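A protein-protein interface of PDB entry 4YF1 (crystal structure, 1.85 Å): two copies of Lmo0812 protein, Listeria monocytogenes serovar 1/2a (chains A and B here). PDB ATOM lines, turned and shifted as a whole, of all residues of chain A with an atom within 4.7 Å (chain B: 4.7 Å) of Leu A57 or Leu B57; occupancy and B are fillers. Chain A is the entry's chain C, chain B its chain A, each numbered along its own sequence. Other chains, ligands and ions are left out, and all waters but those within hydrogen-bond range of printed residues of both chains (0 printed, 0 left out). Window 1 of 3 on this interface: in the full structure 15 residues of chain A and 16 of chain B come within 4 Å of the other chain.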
ATOM      1  N   PRO A  36       6.597  19.106  18.075  1.00  0.00           N
ATOM      2  CA  PRO A  36       5.767  18.067  17.474  1.00  0.00           C
ATOM      3  C   PRO A  36       6.583  16.993  16.756  1.00  0.00           C
ATOM      4  O   PRO A  36       6.284  15.816  16.901  1.00  0.00           O
ATOM      5  CB  PRO A  36       4.893  18.845  16.493  1.00  0.00           C
ATOM      6  CG  PRO A  36       4.722  20.168  17.141  1.00  0.00           C
ATOM      7  CD  PRO A  36       6.038  20.451  17.821  1.00  0.00           C
ATOM      8  N   LEU A  37       7.613  17.397  16.014  1.00  0.00           N
ATOM      9  CA  LEU A  37       8.469  16.439  15.318  1.00  0.00           C
ATOM     10  C   LEU A  37       9.229  15.551  16.293  1.00  0.00           C
ATOM     11  O   LEU A  37       9.464  14.381  16.001  1.00  0.00           O
ATOM     12  CB  LEU A  37       9.435  17.115  14.344  1.00  0.00           C
ATOM     13  CG  LEU A  37       8.834  17.378  12.954  1.00  0.00           C
ATOM     14  CD1 LEU A  37       7.628  18.298  13.009  1.00  0.00           C
ATOM     15  CD2 LEU A  37       9.912  17.943  12.050  1.00  0.00           C
ATOM     16  N   VAL A  39       8.080  14.669  19.294  1.00  0.00           N
ATOM     17  CA  VAL A  39       7.096  13.735  19.809  1.00  0.00           C
ATOM     18  C   VAL A  39       6.903  12.594  18.788  1.00  0.00           C
ATOM     19  O   VAL A  39       6.865  11.427  19.167  1.00  0.00           O
ATOM     20  CB  VAL A  39       5.751  14.412  20.175  1.00  0.00           C
ATOM     21  CG1 VAL A  39       4.707  13.377  20.552  1.00  0.00           C
ATOM     22  CG2 VAL A  39       5.939  15.388  21.323  1.00  0.00           C
ATOM     23  N   ALA A  40       6.829  12.939  17.505  1.00  0.00           N
ATOM     24  CA  ALA A  40       6.671  11.934  16.446  1.00  0.00           C
ATOM     25  C   ALA A  40       7.847  10.940  16.446  1.00  0.00           C
ATOM     26  O   ALA A  40       7.630   9.720  16.413  1.00  0.00           O
ATOM     27  CB  ALA A  40       6.542  12.610  15.087  1.00  0.00           C
ATOM     28  N   VAL A  53       1.603   7.945  15.929  1.00  0.00           N
ATOM     29  CA  VAL A  53       2.665   8.901  15.661  1.00  0.00           C
ATOM     30  C   VAL A  53       2.063  10.224  15.199  1.00  0.00           C
ATOM     31  O   VAL A  53       2.433  11.285  15.678  1.00  0.00           O
ATOM     32  CB  VAL A  53       3.645   8.357  14.591  1.00  0.00           C
ATOM     33  CG1 VAL A  53       4.683   9.404  14.214  1.00  0.00           C
ATOM     34  CG2 VAL A  53       4.336   7.098  15.083  1.00  0.00           C
ATOM     35  N   VAL A  54       1.100  10.151  14.275  1.00  0.00           N
ATOM     36  CA  VAL A  54       0.471  11.352  13.756  1.00  0.00           C
ATOM     37  C   VAL A  54      -0.394  12.046  14.802  1.00  0.00           C
ATOM     38  O   VAL A  54      -0.405  13.277  14.876  1.00  0.00           O
ATOM     39  CB  VAL A  54      -0.284  11.037  12.455  1.00  0.00           C
ATOM     40  CG1 VAL A  54      -1.186  12.189  12.039  1.00  0.00           C
ATOM     41  CG2 VAL A  54       0.739  10.694  11.385  1.00  0.00           C
ATOM     42  N   ALA A  55      -1.122  11.282  15.604  1.00  0.00           N
ATOM     43  CA  ALA A  55      -1.911  11.868  16.671  1.00  0.00           C
ATOM     44  C   ALA A  55      -0.984  12.663  17.643  1.00  0.00           C
ATOM     45  O   ALA A  55      -1.352  13.731  18.155  1.00  0.00           O
ATOM     46  CB  ALA A  55      -2.650  10.787  17.420  1.00  0.00           C
ATOM     47  N   GLY A  56       0.213  12.150  17.872  1.00  0.00           N
ATOM     48  CA  GLY A  56       1.170  12.830  18.763  1.00  0.00           C
ATOM     49  C   GLY A  56       1.615  14.136  18.138  1.00  0.00           C
ATOM     50  O   GLY A  56       1.601  15.200  18.780  1.00  0.00           O
ATOM     51  N   LEU A  57       2.016  14.037  16.873  1.00  0.00           N
ATOM     52  CA  LEU A  57       2.429  15.171  16.068  1.00  0.00           C
ATOM     53  C   LEU A  57       1.398  16.297  16.037  1.00  0.00           C
ATOM     54  O   LEU A  57       1.755  17.462  16.031  1.00  0.00           O
ATOM     55  CB  LEU A  57       2.638  14.687  14.623  1.00  0.00           C
ATOM     56  CG  LEU A  57       3.019  15.741  13.607  1.00  0.00           C
ATOM     57  CD1 LEU A  57       4.500  16.032  13.707  1.00  0.00           C
ATOM     58  CD2 LEU A  57       2.662  15.267  12.222  1.00  0.00           C
ATOM     59  N   LEU A  58       0.125  15.938  15.995  1.00  0.00           N
ATOM     60  CA  LEU A  58      -0.963  16.898  15.869  1.00  0.00           C
ATOM     61  C   LEU A  58      -1.498  17.508  17.146  1.00  0.00           C
ATOM     62  O   LEU A  58      -2.202  18.508  17.079  1.00  0.00           O
ATOM     63  CB  LEU A  58      -2.151  16.256  15.114  1.00  0.00           C
ATOM     64  CG  LEU A  58      -1.965  15.942  13.632  1.00  0.00           C
ATOM     65  CD1 LEU A  58      -3.251  15.302  13.102  1.00  0.00           C
ATOM     66  CD2 LEU A  58      -1.639  17.201  12.847  1.00  0.00           C
ATOM     67  N   HIS A  59      -1.163  16.927  18.298  1.00  0.00           N
ATOM     68  CA  HIS A  59      -1.683  17.395  19.578  1.00  0.00           C
ATOM     69  C   HIS A  59      -1.662  18.935  19.772  1.00  0.00           C
ATOM     70  O   HIS A  59      -2.695  19.527  20.024  1.00  0.00           O
ATOM     71  CB  HIS A  59      -0.947  16.716  20.725  1.00  0.00           C
ATOM     72  CG  HIS A  59      -1.434  17.136  22.076  1.00  0.00           C
ATOM     73  ND1 HIS A  59      -0.766  18.058  22.854  1.00  0.00           N
ATOM     74  CD2 HIS A  59      -2.545  16.791  22.768  1.00  0.00           C
ATOM     75  CE1 HIS A  59      -1.435  18.247  23.980  1.00  0.00           C
ATOM     76  NE2 HIS A  59      -2.516  17.487  23.954  1.00  0.00           N
ATOM     77  N   PHE A  76      -7.558  13.580   8.260  1.00  0.00           N
ATOM     78  CA  PHE A  76      -6.627  12.533   8.608  1.00  0.00           C
ATOM     79  C   PHE A  76      -7.168  11.116   8.803  1.00  0.00           C
ATOM     80  O   PHE A  76      -6.370  10.174   8.946  1.00  0.00           O
ATOM     81  CB  PHE A  76      -5.876  12.966   9.866  1.00  0.00           C
ATOM     82  CG  PHE A  76      -5.132  14.233   9.685  1.00  0.00           C
ATOM     83  CD1 PHE A  76      -3.954  14.251   8.943  1.00  0.00           C
ATOM     84  CD2 PHE A  76      -5.594  15.411  10.236  1.00  0.00           C
ATOM     85  CE1 PHE A  76      -3.258  15.435   8.764  1.00  0.00           C
ATOM     86  CE2 PHE A  76      -4.883  16.604  10.071  1.00  0.00           C
ATOM     87  CZ  PHE A  76      -3.716  16.614   9.332  1.00  0.00           C
ATOM     88  N   PRO B  36      -3.346  12.267   3.443  1.00  0.00           N
ATOM     89  CA  PRO B  36      -2.122  12.744   4.126  1.00  0.00           C
ATOM     90  C   PRO B  36      -1.230  11.622   4.660  1.00  0.00           C
ATOM     91  O   PRO B  36      -0.015  11.726   4.540  1.00  0.00           O
ATOM     92  CB  PRO B  36      -2.665  13.572   5.288  1.00  0.00           C
ATOM     93  CG  PRO B  36      -4.021  14.008   4.851  1.00  0.00           C
ATOM     94  CD  PRO B  36      -4.562  12.852   4.055  1.00  0.00           C
ATOM     95  N   LEU B  37      -1.813  10.583   5.263  1.00  0.00           N
ATOM     96  CA  LEU B  37      -1.035   9.471   5.776  1.00  0.00           C
ATOM     97  C   LEU B  37      -0.344   8.709   4.646  1.00  0.00           C
ATOM     98  O   LEU B  37       0.795   8.307   4.779  1.00  0.00           O
ATOM     99  CB  LEU B  37      -1.909   8.554   6.636  1.00  0.00           C
ATOM    100  CG  LEU B  37      -2.232   9.077   8.045  1.00  0.00           C
ATOM    101  CD1 LEU B  37      -0.986   9.023   8.892  1.00  0.00           C
ATOM    102  CD2 LEU B  37      -2.786  10.482   8.077  1.00  0.00           C
ATOM    103  N   ALA B  40       2.487  10.845   3.278  1.00  0.00           N
ATOM    104  CA  ALA B  40       3.621  10.811   4.270  1.00  0.00           C
ATOM    105  C   ALA B  40       4.421   9.505   4.155  1.00  0.00           C
ATOM    106  O   ALA B  40       5.641   9.503   4.246  1.00  0.00           O
ATOM    107  CB  ALA B  40       3.083  10.999   5.686  1.00  0.00           C
ATOM    108  N   VAL B  53       8.302  14.974   5.398  1.00  0.00           N
ATOM    109  CA  VAL B  53       7.192  14.065   5.613  1.00  0.00           C
ATOM    110  C   VAL B  53       5.990  14.796   6.222  1.00  0.00           C
ATOM    111  O   VAL B  53       4.839  14.623   5.779  1.00  0.00           O
ATOM    112  CB  VAL B  53       7.611  12.878   6.488  1.00  0.00           C
ATOM    113  CG1 VAL B  53       6.396  12.080   6.934  1.00  0.00           C
ATOM    114  CG2 VAL B  53       8.602  12.012   5.739  1.00  0.00           C
ATOM    115  N   VAL B  54       6.260  15.617   7.227  1.00  0.00           N
ATOM    116  CA  VAL B  54       5.209  16.374   7.897  1.00  0.00           C
ATOM    117  C   VAL B  54       4.600  17.421   6.994  1.00  0.00           C
ATOM    118  O   VAL B  54       3.391  17.652   7.059  1.00  0.00           O
ATOM    119  CB  VAL B  54       5.712  16.994   9.209  1.00  0.00           C
ATOM    120  CG1 VAL B  54       4.675  17.936   9.808  1.00  0.00           C
ATOM    121  CG2 VAL B  54       6.034  15.879  10.196  1.00  0.00           C
ATOM    122  N   ALA B  55       5.421  18.063   6.156  1.00  0.00           N
ATOM    123  CA  ALA B  55       4.875  19.040   5.211  1.00  0.00           C
ATOM    124  C   ALA B  55       3.898  18.320   4.287  1.00  0.00           C
ATOM    125  O   ALA B  55       2.859  18.873   3.944  1.00  0.00           O
ATOM    126  CB  ALA B  55       5.974  19.714   4.406  1.00  0.00           C
ATOM    127  N   GLY B  56       4.221  17.078   3.898  1.00  0.00           N
ATOM    128  CA  GLY B  56       3.302  16.315   3.021  1.00  0.00           C
ATOM    129  C   GLY B  56       1.995  16.012   3.736  1.00  0.00           C
ATOM    130  O   GLY B  56       0.894  16.089   3.161  1.00  0.00           O
ATOM    131  N   LEU B  57       2.126  15.653   5.003  1.00  0.00           N
ATOM    132  CA  LEU B  57       0.993  15.361   5.855  1.00  0.00           C
ATOM    133  C   LEU B  57       0.036  16.581   6.018  1.00  0.00           C
ATOM    134  O   LEU B  57      -1.198  16.425   6.019  1.00  0.00           O
ATOM    135  CB  LEU B  57       1.529  14.957   7.234  1.00  0.00           C
ATOM    136  CG  LEU B  57       0.582  14.313   8.213  1.00  0.00           C
ATOM    137  CD1 LEU B  57       0.346  12.857   7.841  1.00  0.00           C
ATOM    138  CD2 LEU B  57       1.166  14.403   9.621  1.00  0.00           C
ATOM    139  N   LEU B  58       0.613  17.782   6.140  1.00  0.00           N
ATOM    140  CA  LEU B  58      -0.178  18.994   6.401  1.00  0.00           C
ATOM    141  C   LEU B  58      -0.796  19.676   5.172  1.00  0.00           C
ATOM    142  O   LEU B  58      -1.625  20.576   5.325  1.00  0.00           O
ATOM    143  CB  LEU B  58       0.663  19.989   7.177  1.00  0.00           C
ATOM    144  CG  LEU B  58       1.095  19.506   8.566  1.00  0.00           C
ATOM    145  CD1 LEU B  58       2.081  20.488   9.177  1.00  0.00           C
ATOM    146  CD2 LEU B  58      -0.095  19.313   9.492  1.00  0.00           C
ATOM    147  N   HIS B  59      -0.422  19.243   3.973  1.00  0.00           N
ATOM    148  CA  HIS B  59      -0.943  19.857   2.755  1.00  0.00           C
ATOM    149  C   HIS B  59      -2.481  19.989   2.747  1.00  0.00           C
ATOM    150  O   HIS B  59      -2.998  21.099   2.576  1.00  0.00           O
ATOM    151  CB  HIS B  59      -0.405  19.120   1.516  1.00  0.00           C
ATOM    152  CG  HIS B  59      -1.061  19.517   0.231  1.00  0.00           C
ATOM    153  ND1 HIS B  59      -0.638  20.586  -0.527  1.00  0.00           N
ATOM    154  CD2 HIS B  59      -2.124  18.988  -0.426  1.00  0.00           C
ATOM    155  CE1 HIS B  59      -1.409  20.698  -1.598  1.00  0.00           C
ATOM    156  NE2 HIS B  59      -2.310  19.733  -1.565  1.00  0.00           N
ATOM    157  N   ASP B  60      -3.195  18.883   2.953  1.00  0.00           N
ATOM    158  CA  ASP B  60      -4.689  18.901   2.966  1.00  0.00           C
ATOM    159  C   ASP B  60      -5.277  19.719   4.113  1.00  0.00           C
ATOM    160  O   ASP B  60      -6.372  20.264   3.979  1.00  0.00           O
ATOM    161  CB  ASP B  60      -5.281  17.491   3.095  1.00  0.00           C
ATOM    162  CG  ASP B  60      -5.132  16.651   1.843  1.00  0.00           C
ATOM    163  OD1 ASP B  60      -4.510  17.085   0.841  1.00  0.00           O
ATOM    164  OD2 ASP B  60      -5.674  15.528   1.877  1.00  0.00           O
ATOM    165  N   PHE B  76       4.600  24.201  14.186  1.00  0.00           N
ATOM    166  CA  PHE B  76       5.653  23.368  13.573  1.00  0.00           C
ATOM    167  C   PHE B  76       6.930  24.091  13.149  1.00  0.00           C
ATOM    168  O   PHE B  76       7.906  23.438  12.783  1.00  0.00           O
ATOM    169  CB  PHE B  76       5.068  22.664  12.345  1.00  0.00           C
ATOM    170  CG  PHE B  76       3.914  21.753  12.664  1.00  0.00           C
ATOM    171  CD1 PHE B  76       4.142  20.450  13.113  1.00  0.00           C
ATOM    172  CD2 PHE B  76       2.609  22.181  12.510  1.00  0.00           C
ATOM    173  CE1 PHE B  76       3.085  19.606  13.410  1.00  0.00           C
ATOM    174  CE2 PHE B  76       1.543  21.340  12.805  1.00  0.00           C
ATOM    175  CZ  PHE B  76       1.781  20.051  13.263  1.00  0.00           C
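Phe B76 touches Pro A36. Val A54 touches Leu B37. Leu A57 touches Val B54 (CD1 to CG2, 3.8 Å). Leu B57 touches Leu A57 (CD2 to CD2, 3.1 Å). Leu A57 touches Phe B76. CD1 of Phe A76 touches CB of Pro B36, at 3.9 Å. Phe A76 touches Leu B37. CE1 of Phe A76 touches O of Leu B57, at 3.6 Å.
Of the printed residues of chain B, Pro A36 touches Phe B76. Leu A57 touches just these residues of chain B: Val B54, Leu B57 and Phe B76. Leu B57 touches just these residues of chain A: Leu A57 (3.1 Å) and Phe A76 (3.6 Å). Printed residues of chain A within 4 Å of Phe B76: Pro A36 (3.7 Å) and Leu A57 (3.6 Å). The nearest printed residue of chain B that does not touch Leu A57 is Leu B58 (5.6 Å). The nearest residue of chain A that does not touch Leu B57 is Val A54 (4.03 Å).
Of the 12 printed residues of chain B, 5 touch a printed residue of chain A. Hydrophobic or aromatic side chains of chain B within 4 Å of the printed part of chain A: Pro B36, Leu B37, Val B54, Leu B57 and Phe B76. Of the 12 printed residues of chain A, 4 touch a printed residue of chain B. Among the printed residues, 8 pairs touch across the chains.
Pro A36 touches Phe B76, and with the chains exchanged Phe A76 touches Pro B36. Leu A57 touches Val B54, but with the chains exchanged Val A54 does not touch Leu B57 (4.03 Å). Leu B57 touches its own counterpart, Leu A57. Phe A76 touches Leu B37, but with the chains exchanged Leu A37 does not touch Phe B76 (4.1 Å). 11 positions are printed for both chains. Of the 8 pairs that touch across the chains among the printed residues, 5 have their exchanged pair printed and touching as well.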
